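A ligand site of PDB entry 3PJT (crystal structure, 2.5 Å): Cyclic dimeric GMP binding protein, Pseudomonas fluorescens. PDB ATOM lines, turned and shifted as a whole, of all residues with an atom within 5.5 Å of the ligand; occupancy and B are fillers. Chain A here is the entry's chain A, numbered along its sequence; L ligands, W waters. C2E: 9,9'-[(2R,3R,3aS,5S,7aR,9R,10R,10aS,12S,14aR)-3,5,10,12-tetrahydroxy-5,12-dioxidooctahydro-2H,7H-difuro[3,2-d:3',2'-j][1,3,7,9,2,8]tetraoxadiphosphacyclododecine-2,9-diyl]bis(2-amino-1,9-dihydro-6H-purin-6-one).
The backbone NH (N) of Gln 240 is in hydrogen-bond range of the backbone carbonyl oxygen (O) of Val 220.
The backbone carbonyl oxygen (O) of Glu 132 sits close to the side-chain amide nitrogen (ND2) of Asn 100, at 3.4 Å.
The backbone NH (N) of Ala 62 is in hydrogen-bond range of the backbone carbonyl oxygen (O) of Ser 50 (3.3 Å).
OE2 of Glu 218 lies within hydrogen-bond range of N of Arg 162 (2.8 Å).
The backbone carbonyl oxygen (O) of Val 220 is in hydrogen-bond range of the backbone NH (N) of Leu 241, 3.1 Å away.
The side-chain carboxylate (OE1) of Glu 221 lies within salt-bridge range of the guanidinium group (NH1) of Arg 189 (3.3 Å).
The backbone NH of Lys 47 lies within hydrogen-bond range of the backbone carbonyl oxygen of Gln 32, at 2.9 Å.
NZ of Lys 47 sits at hydrogen-bond distance from OE1 of Gln 161, at 3.0 Å.
The side-chain sulfur (SD) of Met 82 lies close to an oxygen (O61) of the ligand.
Merely in contact with the ligand: Leu 49, Pro 61, Leu 66, Leu 78, Ser 102, Val 220, Gln 238, Gly 239 and Pro 245.
Hydrophobic or aromatic side chains that line the ligand: Leu 49, Pro 61, Ala 62, Leu 66, Leu 78, Met 82 and Pro 245.
23 residues have an atom within 4 Å of the ligand: Gln 32, Lys 47, Leu 49, Ser 50, Arg 51, Pro 61, Ala 62, Gly 63, Leu 66, Leu 78, Asp 79, Met 82, Asn 100, Ser 102, Gln 161, Arg 162, Arg 219, Val 220, Glu 221, Gln 238, Gly 239, Gln 240 and Pro 245.
Water W6 lies within hydrogen-bond range of a nitrogen (N11) of the ligand (2.7 Å), the side-chain carboxylate (OD1) of Asp 79 (2.7 Å) and the backbone carbonyl oxygen (O) of Asn 100 (2.9 Å).
Water W5 lies within hydrogen-bond range of O1P of the ligand (2.8 Å), OE1 of Glu 218 (2.8 Å), NH1 of Arg 162 (2.9 Å) and NH2 of Arg 219 (3.0 Å).
Water W7 lies within hydrogen-bond range of NE2 of Gln 238 (2.7 Å) and O1P of the ligand (2.9 Å).
Water W4 lies within hydrogen-bond range of the side-chain amide oxygen (OE1) of Gln 32 (2.9 Å) and an oxygen (O5') of the ligand (2.9 Å).
Water W3 lies within hydrogen-bond range of the side-chain amide nitrogen of Gln 240 (3.0 Å) and an oxygen (O2') of the ligand (3.1 Å).
The guanidinium group (NH1) of Arg 162 is in salt-bridge range of an oxygen (O1P) of the ligand, at 3.9 Å.
The guanidinium group of Arg 219 is in hydrogen-bond range of an oxygen (O4') of the ligand.
NE2 of Gln 240 lies within hydrogen-bond range of N3 of the ligand (3.4 Å).
N1 of the ligand is in hydrogen-bond range of OE2 of Glu 221 (2.7 Å).
An oxygen (O6) of the ligand is in hydrogen-bond range of the backbone NH of Gln 240, at 2.7 Å.
A nitrogen (N21) of the ligand sits at hydrogen-bond distance from the side-chain carboxylate (OD1) of Asp 79 (3.2 Å).
OE1 of Gln 161 is in hydrogen-bond range of O2A of the ligand, 2.7 Å away.
A nitrogen (N7) of the ligand sits close to the side-chain amide nitrogen of Gln 32 (3.3 Å).
The side-chain amino group of Lys 47 is in salt-bridge range of an oxygen (O2P) of the ligand (2.5 Å).
The backbone NH of Gly 63 is in hydrogen-bond range of an oxygen (O11) of the ligand (2.9 Å).
The guanidinium group (NH2) of Arg 51 is in salt-bridge range of an oxygen (O21) of the ligand.
OD1 of Asn 100 sits at hydrogen-bond distance from O2A of the ligand (3.2 Å).
The backbone NH (N) of Ala 62 lies within hydrogen-bond range of an oxygen (O11) of the ligand (3.5 Å).
N71 of the ligand sits at hydrogen-bond distance from N of Ser 50 (3.0 Å).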
ATOM      1  N   GLN A  32       2.450  -0.864  27.816  1.00  0.00           N
ATOM      2  CA  GLN A  32       1.018  -0.685  27.768  1.00  0.00           C
ATOM      3  C   GLN A  32       0.451  -1.401  28.995  1.00  0.00           C
ATOM      4  O   GLN A  32       0.699  -2.601  29.222  1.00  0.00           O
ATOM      5  CB  GLN A  32       0.443  -1.267  26.484  1.00  0.00           C
ATOM      6  CG  GLN A  32      -0.879  -0.661  26.105  1.00  0.00           C
ATOM      7  CD  GLN A  32      -1.340  -1.102  24.736  1.00  0.00           C
ATOM      8  OE1 GLN A  32      -0.853  -2.112  24.203  1.00  0.00           O
ATOM      9  NE2 GLN A  32      -2.296  -0.369  24.163  1.00  0.00           N
ATOM     10  N   LYS A  47       2.681  -4.624  29.932  1.00  0.00           N
ATOM     11  CA  LYS A  47       3.210  -5.440  28.861  1.00  0.00           C
ATOM     12  C   LYS A  47       4.332  -4.670  28.162  1.00  0.00           C
ATOM     13  O   LYS A  47       4.112  -3.516  27.755  1.00  0.00           O
ATOM     14  CB  LYS A  47       2.104  -5.757  27.844  1.00  0.00           C
ATOM     15  CG  LYS A  47       2.524  -6.740  26.744  1.00  0.00           C
ATOM     16  CD  LYS A  47       2.957  -8.133  27.309  1.00  0.00           C
ATOM     17  CE  LYS A  47       3.296  -9.094  26.194  1.00  0.00           C
ATOM     18  NZ  LYS A  47       2.103  -9.346  25.318  1.00  0.00           N
ATOM     19  N   VAL A  48       5.512  -5.290  28.053  1.00  0.00           N
ATOM     20  CA  VAL A  48       6.605  -4.697  27.287  1.00  0.00           C
ATOM     21  C   VAL A  48       6.377  -4.902  25.778  1.00  0.00           C
ATOM     22  O   VAL A  48       6.077  -6.002  25.325  1.00  0.00           O
ATOM     23  CB  VAL A  48       7.998  -5.245  27.711  1.00  0.00           C
ATOM     24  CG1 VAL A  48       9.108  -4.628  26.888  1.00  0.00           C
ATOM     25  CG2 VAL A  48       8.271  -5.019  29.193  1.00  0.00           C
ATOM     26  N   LEU A  49       6.491  -3.823  25.024  1.00  0.00           N
ATOM     27  CA  LEU A  49       6.360  -3.826  23.584  1.00  0.00           C
ATOM     28  C   LEU A  49       7.705  -3.388  23.000  1.00  0.00           C
ATOM     29  O   LEU A  49       8.326  -2.443  23.467  1.00  0.00           O
ATOM     30  CB  LEU A  49       5.269  -2.834  23.164  1.00  0.00           C
ATOM     31  CG  LEU A  49       3.832  -3.298  22.919  1.00  0.00           C
ATOM     32  CD1 LEU A  49       3.612  -4.743  23.239  1.00  0.00           C
ATOM     33  CD2 LEU A  49       2.845  -2.428  23.664  1.00  0.00           C
ATOM     34  N   SER A  50       8.195  -4.090  21.983  1.00  0.00           N
ATOM     35  CA  SER A  50       9.450  -3.694  21.379  1.00  0.00           C
ATOM     36  C   SER A  50       9.203  -2.617  20.330  1.00  0.00           C
ATOM     37  O   SER A  50       8.234  -2.704  19.573  1.00  0.00           O
ATOM     38  CB  SER A  50      10.188  -4.889  20.764  1.00  0.00           C
ATOM     39  OG  SER A  50      11.463  -4.475  20.357  1.00  0.00           O
ATOM     40  N   ARG A  51      10.082  -1.617  20.294  1.00  0.00           N
ATOM     41  CA  ARG A  51      10.022  -0.569  19.283  1.00  0.00           C
ATOM     42  C   ARG A  51      11.397  -0.416  18.617  1.00  0.00           C
ATOM     43  O   ARG A  51      12.406  -0.125  19.287  1.00  0.00           O
ATOM     44  CB  ARG A  51       9.550   0.777  19.851  1.00  0.00           C
ATOM     45  CG  ARG A  51       8.067   0.848  20.257  1.00  0.00           C
ATOM     46  CD  ARG A  51       7.126   0.802  19.058  1.00  0.00           C
ATOM     47  NE  ARG A  51       6.036  -0.150  19.269  1.00  0.00           N
ATOM     48  CZ  ARG A  51       4.754   0.185  19.401  1.00  0.00           C
ATOM     49  NH1 ARG A  51       4.373   1.462  19.323  1.00  0.00           N
ATOM     50  NH2 ARG A  51       3.847  -0.773  19.587  1.00  0.00           N
ATOM     51  N   PRO A  61       6.750  -0.095  15.202  1.00  0.00           N
ATOM     52  CA  PRO A  61       6.086  -1.026  16.129  1.00  0.00           C
ATOM     53  C   PRO A  61       6.404  -2.500  15.813  1.00  0.00           C
ATOM     54  O   PRO A  61       6.630  -2.819  14.637  1.00  0.00           O
ATOM     55  CB  PRO A  61       4.595  -0.714  15.951  1.00  0.00           C
ATOM     56  CG  PRO A  61       4.492  -0.138  14.577  1.00  0.00           C
ATOM     57  CD  PRO A  61       5.813   0.494  14.222  1.00  0.00           C
ATOM     58  N   ALA A  62       6.453  -3.369  16.825  1.00  0.00           N
ATOM     59  CA  ALA A  62       6.703  -4.795  16.625  1.00  0.00           C
ATOM     60  C   ALA A  62       5.794  -5.404  15.548  1.00  0.00           C
ATOM     61  O   ALA A  62       6.239  -6.227  14.734  1.00  0.00           O
ATOM     62  CB  ALA A  62       6.557  -5.544  17.924  1.00  0.00           C
ATOM     63  N   GLY A  63       4.529  -4.986  15.551  1.00  0.00           N
ATOM     64  CA  GLY A  63       3.562  -5.461  14.584  1.00  0.00           C
ATOM     65  C   GLY A  63       4.074  -5.450  13.163  1.00  0.00           C
ATOM     66  O   GLY A  63       3.787  -6.332  12.352  1.00  0.00           O
ATOM     67  N   ARG A  64       4.856  -4.431  12.844  1.00  0.00           N
ATOM     68  CA  ARG A  64       5.285  -4.220  11.453  1.00  0.00           C
ATOM     69  C   ARG A  64       6.612  -4.915  11.148  1.00  0.00           C
ATOM     70  O   ARG A  64       6.822  -5.382  10.036  1.00  0.00           O
ATOM     71  CB  ARG A  64       5.323  -2.714  11.128  1.00  0.00           C
ATOM     72  CG  ARG A  64       6.309  -2.296  10.059  1.00  0.00           C
ATOM     73  CD  ARG A  64       5.612  -1.837   8.785  1.00  0.00           C
ATOM     74  NE  ARG A  64       5.807  -2.785   7.677  1.00  0.00           N
ATOM     75  CZ  ARG A  64       6.237  -2.432   6.459  1.00  0.00           C
ATOM     76  NH1 ARG A  64       6.493  -1.155   6.187  1.00  0.00           N
ATOM     77  NH2 ARG A  64       6.387  -3.357   5.515  1.00  0.00           N
ATOM     78  N   LEU A  66       8.104  -7.515  13.041  1.00  0.00           N
ATOM     79  CA  LEU A  66       8.202  -8.918  13.465  1.00  0.00           C
ATOM     80  C   LEU A  66       8.095  -9.925  12.310  1.00  0.00           C
ATOM     81  O   LEU A  66       8.850 -10.886  12.265  1.00  0.00           O
ATOM     82  CB  LEU A  66       7.183  -9.236  14.557  1.00  0.00           C
ATOM     83  CG  LEU A  66       7.666  -8.871  15.964  1.00  0.00           C
ATOM     84  CD1 LEU A  66       6.533  -9.011  16.971  1.00  0.00           C
ATOM     85  CD2 LEU A  66       8.868  -9.726  16.349  1.00  0.00           C
ATOM     86  N   THR A  75      14.379 -13.846  15.136  1.00  0.00           N
ATOM     87  CA  THR A  75      13.537 -13.584  16.290  1.00  0.00           C
ATOM     88  C   THR A  75      14.253 -13.875  17.607  1.00  0.00           C
ATOM     89  O   THR A  75      14.067 -13.173  18.586  1.00  0.00           O
ATOM     90  CB  THR A  75      12.222 -14.324  16.214  1.00  0.00           C
ATOM     91  OG1 THR A  75      11.910 -14.589  14.844  1.00  0.00           O
ATOM     92  CG2 THR A  75      11.146 -13.463  16.773  1.00  0.00           C
ATOM     93  N   LEU A  78      16.180 -10.860  18.815  1.00  0.00           N
ATOM     94  CA  LEU A  78      15.328  -9.905  19.481  1.00  0.00           C
ATOM     95  C   LEU A  78      15.059 -10.380  20.905  1.00  0.00           C
ATOM     96  O   LEU A  78      15.299  -9.651  21.875  1.00  0.00           O
ATOM     97  CB  LEU A  78      14.014  -9.731  18.736  1.00  0.00           C
ATOM     98  CG  LEU A  78      13.070  -8.764  19.435  1.00  0.00           C
ATOM     99  CD1 LEU A  78      13.541  -7.318  19.269  1.00  0.00           C
ATOM    100  CD2 LEU A  78      11.690  -8.954  18.889  1.00  0.00           C
ATOM    101  N   ASP A  79      14.560 -11.608  21.016  1.00  0.00           N
ATOM    102  CA  ASP A  79      14.233 -12.171  22.303  1.00  0.00           C
ATOM    103  C   ASP A  79      15.345 -11.961  23.351  1.00  0.00           C
ATOM    104  O   ASP A  79      15.064 -11.476  24.461  1.00  0.00           O
ATOM    105  CB  ASP A  79      13.894 -13.657  22.185  1.00  0.00           C
ATOM    106  CG  ASP A  79      12.471 -13.908  21.698  1.00  0.00           C
ATOM    107  OD1 ASP A  79      11.687 -12.939  21.597  1.00  0.00           O
ATOM    108  OD2 ASP A  79      12.141 -15.078  21.423  1.00  0.00           O
ATOM    109  N   MET A  82      15.854  -8.117  24.103  1.00  0.00           N
ATOM    110  CA  MET A  82      14.718  -7.606  24.854  1.00  0.00           C
ATOM    111  C   MET A  82      14.710  -8.096  26.289  1.00  0.00           C
ATOM    112  O   MET A  82      14.494  -7.314  27.218  1.00  0.00           O
ATOM    113  CB  MET A  82      13.409  -7.997  24.169  1.00  0.00           C
ATOM    114  CG  MET A  82      13.174  -7.263  22.873  1.00  0.00           C
ATOM    115  SD  MET A  82      12.819  -5.481  23.069  1.00  0.00           S
ATOM    116  CE  MET A  82      11.481  -5.568  24.264  1.00  0.00           C
ATOM    117  N   LEU A  99       6.412 -10.202  29.104  1.00  0.00           N
ATOM    118  CA  LEU A  99       7.268 -10.194  27.930  1.00  0.00           C
ATOM    119  C   LEU A  99       7.121 -11.479  27.143  1.00  0.00           C
ATOM    120  O   LEU A  99       7.133 -12.572  27.727  1.00  0.00           O
ATOM    121  CB  LEU A  99       8.739 -10.069  28.324  1.00  0.00           C
ATOM    122  CG  LEU A  99       9.715 -10.076  27.146  1.00  0.00           C
ATOM    123  CD1 LEU A  99       9.420  -8.830  26.328  1.00  0.00           C
ATOM    124  CD2 LEU A  99      11.196 -10.112  27.581  1.00  0.00           C
ATOM    125  N   ASN A 100       7.002 -11.330  25.826  1.00  0.00           N
ATOM    126  CA  ASN A 100       6.897 -12.441  24.889  1.00  0.00           C
ATOM    127  C   ASN A 100       8.207 -13.191  24.661  1.00  0.00           C
ATOM    128  O   ASN A 100       9.241 -12.561  24.508  1.00  0.00           O
ATOM    129  CB  ASN A 100       6.390 -11.934  23.541  1.00  0.00           C
ATOM    130  CG  ASN A 100       4.917 -11.609  23.537  1.00  0.00           C
ATOM    131  OD1 ASN A 100       4.514 -10.480  23.785  1.00  0.00           O
ATOM    132  ND2 ASN A 100       4.089 -12.627  23.274  1.00  0.00           N
ATOM    133  N   LEU A 101       8.143 -14.530  24.657  1.00  0.00           N
ATOM    134  CA  LEU A 101       9.169 -15.353  23.999  1.00  0.00           C
ATOM    135  C   LEU A 101       8.668 -15.859  22.646  1.00  0.00           C
ATOM    136  O   LEU A 101       7.478 -16.161  22.495  1.00  0.00           O
ATOM    137  CB  LEU A 101       9.603 -16.511  24.895  1.00  0.00           C
ATOM    138  CG  LEU A 101      10.686 -16.128  25.897  1.00  0.00           C
ATOM    139  CD1 LEU A 101      11.588 -15.042  25.355  1.00  0.00           C
ATOM    140  CD2 LEU A 101      10.056 -15.638  27.168  1.00  0.00           C
ATOM    141  N   SER A 102       9.545 -15.927  21.655  1.00  0.00           N
ATOM    142  CA  SER A 102       9.133 -16.369  20.322  1.00  0.00           C
ATOM    143  C   SER A 102       9.341 -17.883  20.149  1.00  0.00           C
ATOM    144  O   SER A 102      10.140 -18.497  20.863  1.00  0.00           O
ATOM    145  CB  SER A 102       9.903 -15.597  19.257  1.00  0.00           C
ATOM    146  OG  SER A 102      11.280 -15.901  19.293  1.00  0.00           O
ATOM    147  N   GLU A 132       5.300 -14.602  28.036  1.00  0.00           N
ATOM    148  CA  GLU A 132       4.107 -14.863  27.245  1.00  0.00           C
ATOM    149  C   GLU A 132       4.418 -15.538  25.918  1.00  0.00           C
ATOM    150  O   GLU A 132       5.349 -15.130  25.210  1.00  0.00           O
ATOM    151  CB  GLU A 132       3.327 -13.570  26.986  1.00  0.00           C
ATOM    152  CG  GLU A 132       2.535 -13.068  28.174  1.00  0.00           C
ATOM    153  CD  GLU A 132       1.651 -11.853  27.858  1.00  0.00           C
ATOM    154  OE1 GLU A 132       1.432 -11.531  26.672  1.00  0.00           O
ATOM    155  OE2 GLU A 132       1.154 -11.223  28.808  1.00  0.00           O
ATOM    156  N   GLN A 161      -1.133 -15.807  25.181  1.00  0.00           N
ATOM    157  CA  GLN A 161      -1.917 -14.661  24.728  1.00  0.00           C
ATOM    158  C   GLN A 161      -2.510 -14.921  23.352  1.00  0.00           C
ATOM    159  O   GLN A 161      -2.204 -15.942  22.729  1.00  0.00           O
ATOM    160  CB  GLN A 161      -1.098 -13.360  24.765  1.00  0.00           C
ATOM    161  CG  GLN A 161      -0.028 -13.196  23.685  1.00  0.00           C
ATOM    162  CD  GLN A 161       0.332 -11.698  23.432  1.00  0.00           C
ATOM    163  OE1 GLN A 161       1.481 -11.364  23.181  1.00  0.00           O
ATOM    164  NE2 GLN A 161      -0.665 -10.819  23.512  1.00  0.00           N
ATOM    165  N   ARG A 162      -3.374 -14.018  22.887  1.00  0.00           N
ATOM    166  CA  ARG A 162      -4.100 -14.215  21.649  1.00  0.00           C
ATOM    167  C   ARG A 162      -4.849 -15.557  21.623  1.00  0.00           C
ATOM    168  O   ARG A 162      -4.988 -16.204  20.604  1.00  0.00           O
ATOM    169  CB  ARG A 162      -3.157 -14.085  20.433  1.00  0.00           C
ATOM    170  CG  ARG A 162      -2.714 -12.654  20.194  1.00  0.00           C
ATOM    171  CD  ARG A 162      -2.010 -12.511  18.870  1.00  0.00           C
ATOM    172  NE  ARG A 162      -0.612 -12.921  18.963  1.00  0.00           N
ATOM    173  CZ  ARG A 162       0.331 -12.195  19.550  1.00  0.00           C
ATOM    174  NH1 ARG A 162       0.010 -11.022  20.088  1.00  0.00           N
ATOM    175  NH2 ARG A 162       1.583 -12.646  19.605  1.00  0.00           N
ATOM    176  N   ARG A 189     -14.140  -8.055  20.016  1.00  0.00           N
ATOM    177  CA  ARG A 189     -14.418  -6.893  19.190  1.00  0.00           C
ATOM    178  C   ARG A 189     -15.906  -6.599  18.960  1.00  0.00           C
ATOM    179  O   ARG A 189     -16.655  -7.421  18.401  1.00  0.00           O
ATOM    180  CB  ARG A 189     -13.704  -6.987  17.863  1.00  0.00           C
ATOM    181  CG  ARG A 189     -13.966  -5.791  16.969  1.00  0.00           C
ATOM    182  CD  ARG A 189     -13.222  -4.543  17.464  1.00  0.00           C
ATOM    183  NE  ARG A 189     -11.796  -4.809  17.644  1.00  0.00           N
ATOM    184  CZ  ARG A 189     -11.115  -4.596  18.774  1.00  0.00           C
ATOM    185  NH1 ARG A 189     -11.716  -4.076  19.834  1.00  0.00           N
ATOM    186  NH2 ARG A 189      -9.816  -4.882  18.828  1.00  0.00           N
ATOM    187  N   GLU A 218      -7.840  -8.865  25.423  1.00  0.00           N
ATOM    188  CA  GLU A 218      -6.894  -8.012  24.700  1.00  0.00           C
ATOM    189  C   GLU A 218      -7.587  -6.987  23.800  1.00  0.00           C
ATOM    190  O   GLU A 218      -8.712  -7.193  23.358  1.00  0.00           O
ATOM    191  CB  GLU A 218      -5.965  -8.853  23.821  1.00  0.00           C
ATOM    192  CG  GLU A 218      -5.054  -9.815  24.572  1.00  0.00           C
ATOM    193  CD  GLU A 218      -4.231 -10.689  23.637  1.00  0.00           C
ATOM    194  OE1 GLU A 218      -4.328 -10.561  22.400  1.00  0.00           O
ATOM    195  OE2 GLU A 218      -3.466 -11.514  24.145  1.00  0.00           O
ATOM    196  N   ARG A 219      -6.891  -5.880  23.540  1.00  0.00           N
ATOM    197  CA  ARG A 219      -7.311  -4.878  22.559  1.00  0.00           C
ATOM    198  C   ARG A 219      -8.720  -4.340  22.739  1.00  0.00           C
ATOM    199  O   ARG A 219      -9.449  -4.195  21.793  1.00  0.00           O
ATOM    200  CB  ARG A 219      -7.093  -5.410  21.143  1.00  0.00           C
ATOM    201  CG  ARG A 219      -5.636  -5.644  20.819  1.00  0.00           C
ATOM    202  CD  ARG A 219      -5.460  -6.210  19.409  1.00  0.00           C
ATOM    203  NE  ARG A 219      -4.251  -7.025  19.273  1.00  0.00           N
ATOM    204  CZ  ARG A 219      -3.305  -6.825  18.354  1.00  0.00           C
ATOM    205  NH1 ARG A 219      -3.420  -5.832  17.492  1.00  0.00           N
ATOM    206  NH2 ARG A 219      -2.235  -7.610  18.321  1.00  0.00           N
ATOM    207  N   VAL A 220      -9.092  -4.080  23.982  1.00  0.00           N
ATOM    208  CA  VAL A 220     -10.369  -3.468  24.322  1.00  0.00           C
ATOM    209  C   VAL A 220     -10.341  -2.002  23.919  1.00  0.00           C
ATOM    210  O   VAL A 220      -9.493  -1.241  24.402  1.00  0.00           O
ATOM    211  CB  VAL A 220     -10.643  -3.599  25.828  1.00  0.00           C
ATOM    212  CG1 VAL A 220     -11.923  -2.884  26.243  1.00  0.00           C
ATOM    213  CG2 VAL A 220     -10.686  -5.065  26.205  1.00  0.00           C
ATOM    214  N   GLU A 221     -11.251  -1.627  23.026  1.00  0.00           N
ATOM    215  CA  GLU A 221     -11.238  -0.309  22.393  1.00  0.00           C
ATOM    216  C   GLU A 221     -12.329   0.628  22.897  1.00  0.00           C
ATOM    217  O   GLU A 221     -12.237   1.831  22.738  1.00  0.00           O
ATOM    218  CB  GLU A 221     -11.350  -0.462  20.881  1.00  0.00           C
ATOM    219  CG  GLU A 221     -10.014  -0.778  20.231  1.00  0.00           C
ATOM    220  CD  GLU A 221     -10.151  -1.256  18.797  1.00  0.00           C
ATOM    221  OE1 GLU A 221     -11.277  -1.210  18.267  1.00  0.00           O
ATOM    222  OE2 GLU A 221      -9.136  -1.672  18.199  1.00  0.00           O
ATOM    223  N   GLN A 238      -6.949  -4.960  28.528  1.00  0.00           N
ATOM    224  CA  GLN A 238      -5.927  -4.059  27.999  1.00  0.00           C
ATOM    225  C   GLN A 238      -6.413  -3.551  26.658  1.00  0.00           C
ATOM    226  O   GLN A 238      -7.211  -4.233  25.993  1.00  0.00           O
ATOM    227  CB  GLN A 238      -4.556  -4.761  27.866  1.00  0.00           C
ATOM    228  CG  GLN A 238      -4.374  -5.610  26.619  1.00  0.00           C
ATOM    229  CD  GLN A 238      -3.990  -4.811  25.388  1.00  0.00           C
ATOM    230  OE1 GLN A 238      -3.438  -3.716  25.501  1.00  0.00           O
ATOM    231  NE2 GLN A 238      -4.251  -5.353  24.217  1.00  0.00           N
ATOM    232  N   GLY A 239      -5.957  -2.364  26.281  1.00  0.00           N
ATOM    233  CA  GLY A 239      -6.299  -1.865  24.964  1.00  0.00           C
ATOM    234  C   GLY A 239      -6.287  -0.354  24.852  1.00  0.00           C
ATOM    235  O   GLY A 239      -6.051   0.376  25.831  1.00  0.00           O
ATOM    236  N   GLN A 240      -6.558   0.108  23.641  1.00  0.00           N
ATOM    237  CA  GLN A 240      -6.525   1.533  23.333  1.00  0.00           C
ATOM    238  C   GLN A 240      -7.504   2.376  24.176  1.00  0.00           C
ATOM    239  O   GLN A 240      -7.284   3.576  24.363  1.00  0.00           O
ATOM    240  CB  GLN A 240      -6.760   1.731  21.844  1.00  0.00           C
ATOM    241  CG  GLN A 240      -5.494   1.511  21.017  1.00  0.00           C
ATOM    242  CD  GLN A 240      -5.775   1.226  19.552  1.00  0.00           C
ATOM    243  OE1 GLN A 240      -6.906   1.360  19.096  1.00  0.00           O
ATOM    244  NE2 GLN A 240      -4.746   0.820  18.822  1.00  0.00           N
ATOM    245  N   LEU A 241      -8.547   1.738  24.694  1.00  0.00           N
ATOM    246  CA  LEU A 241      -9.455   2.423  25.608  1.00  0.00           C
ATOM    247  C   LEU A 241      -8.691   3.068  26.765  1.00  0.00           C
ATOM    248  O   LEU A 241      -9.100   4.128  27.261  1.00  0.00           O
ATOM    249  CB  LEU A 241     -10.510   1.462  26.166  1.00  0.00           C
ATOM    250  CG  LEU A 241     -11.530   2.140  27.064  1.00  0.00           C
ATOM    251  CD1 LEU A 241     -12.112   3.315  26.288  1.00  0.00           C
ATOM    252  CD2 LEU A 241     -12.607   1.196  27.510  1.00  0.00           C
ATOM    253  N   PRO A 245       0.530   2.644  23.591  1.00  0.00           N
ATOM    254  CA  PRO A 245       1.791   2.194  24.154  1.00  0.00           C
ATOM    255  C   PRO A 245       2.777   3.366  24.252  1.00  0.00           C
ATOM    256  O   PRO A 245       2.836   4.183  23.337  1.00  0.00           O
ATOM    257  CB  PRO A 245       2.268   1.174  23.135  1.00  0.00           C
ATOM    258  CG  PRO A 245       1.010   0.687  22.473  1.00  0.00           C
ATOM    259  CD  PRO A 245       0.122   1.869  22.408  1.00  0.00           C
HETATM  260  P1  C2E L   1       0.542  -7.464  22.290  1.00  0.00           P
HETATM  261  O2P C2E L   1       1.448  -7.900  23.412  1.00  0.00           O
HETATM  262  O1P C2E L   1      -0.824  -8.080  22.537  1.00  0.00           O
HETATM  263  O5' C2E L   1       0.445  -5.875  22.323  1.00  0.00           O
HETATM  264  C5' C2E L   1      -0.638  -5.271  21.675  1.00  0.00           C
HETATM  265  C4' C2E L   1      -0.372  -4.890  20.247  1.00  0.00           C
HETATM  266  O4' C2E L   1      -1.539  -4.439  19.651  1.00  0.00           O
HETATM  267  C3' C2E L   1       0.553  -3.715  20.052  1.00  0.00           C
HETATM  268  O3' C2E L   1       0.986  -3.697  18.741  1.00  0.00           O
HETATM  269  C2' C2E L   1      -0.295  -2.618  20.270  1.00  0.00           C
HETATM  270  O2' C2E L   1       0.097  -1.411  19.652  1.00  0.00           O
HETATM  271  C1' C2E L   1      -1.576  -3.026  19.751  1.00  0.00           C
HETATM  272  N9  C2E L   1      -2.908  -2.568  20.490  1.00  0.00           N
HETATM  273  C8  C2E L   1      -3.001  -2.350  21.811  1.00  0.00           C
HETATM  274  N7  C2E L   1      -4.276  -2.068  22.090  1.00  0.00           N
HETATM  275  C5  C2E L   1      -5.000  -2.123  20.951  1.00  0.00           C
HETATM  276  C6  C2E L   1      -6.355  -1.910  20.688  1.00  0.00           C
HETATM  277  O6  C2E L   1      -7.258  -1.615  21.676  1.00  0.00           O
HETATM  278  N1  C2E L   1      -6.780  -2.027  19.423  1.00  0.00           N
HETATM  279  C2  C2E L   1      -5.908  -2.337  18.445  1.00  0.00           C
HETATM  280  N2  C2E L   1      -6.400  -2.408  17.117  1.00  0.00           N
HETATM  281  N3  C2E L   1      -4.601  -2.557  18.682  1.00  0.00           N
HETATM  282  C4  C2E L   1      -4.119  -2.460  19.923  1.00  0.00           C
HETATM  283  P11 C2E L   1       2.511  -3.963  18.490  1.00  0.00           P
HETATM  284  O21 C2E L   1       3.316  -3.500  19.667  1.00  0.00           O
HETATM  285  O11 C2E L   1       2.982  -3.244  17.253  1.00  0.00           O
HETATM  286  O5A C2E L   1       2.808  -5.457  18.199  1.00  0.00           O
HETATM  287  C5A C2E L   1       3.004  -6.143  19.347  1.00  0.00           C
HETATM  288  C4A C2E L   1       2.633  -7.559  19.273  1.00  0.00           C
HETATM  289  O4A C2E L   1       3.827  -8.320  18.870  1.00  0.00           O
HETATM  290  C3A C2E L   1       2.381  -7.854  20.687  1.00  0.00           C
HETATM  291  O3A C2E L   1       1.043  -8.073  20.932  1.00  0.00           O
HETATM  292  C2A C2E L   1       3.343  -8.894  21.106  1.00  0.00           C
HETATM  293  O2A C2E L   1       2.771 -10.123  21.182  1.00  0.00           O
HETATM  294  C1A C2E L   1       4.393  -8.844  20.037  1.00  0.00           C
HETATM  295  N91 C2E L   1       5.774  -8.259  20.520  1.00  0.00           N
HETATM  296  C81 C2E L   1       5.990  -6.980  20.866  1.00  0.00           C
HETATM  297  N71 C2E L   1       7.227  -6.875  21.374  1.00  0.00           N
HETATM  298  C51 C2E L   1       7.803  -8.094  21.348  1.00  0.00           C
HETATM  299  C61 C2E L   1       9.042  -8.593  21.745  1.00  0.00           C
HETATM  300  O61 C2E L   1       9.953  -7.733  22.335  1.00  0.00           O
HETATM  301  N11 C2E L   1       9.307  -9.910  21.594  1.00  0.00           N
HETATM  302  C21 C2E L   1       8.404 -10.734  21.060  1.00  0.00           C
HETATM  303  N21 C2E L   1       8.713 -12.134  20.890  1.00  0.00           N
HETATM  304  N31 C2E L   1       7.203 -10.268  20.685  1.00  0.00           N
HETATM  305  C41 C2E L   1       6.876  -8.977  20.814  1.00  0.00           C
HETATM  306  O   HOH W   1       0.903  -2.833  15.616  1.00  0.00           O
HETATM  307  O   HOH W   2       6.743  -8.584  24.272  1.00  0.00           O
HETATM  308  O   HOH W   3      -2.070   0.753  20.241  1.00  0.00           O
HETATM  309  O   HOH W   4      -0.055  -4.764  24.936  1.00  0.00           O
HETATM  310  O   HOH W   5      -2.355  -9.480  20.722  1.00  0.00           O
HETATM  311  O   HOH W   6      11.187 -10.867  23.248  1.00  0.00           O
HETATM  312  O   HOH W   7      -2.923  -7.660  24.457  1.00  0.00           O
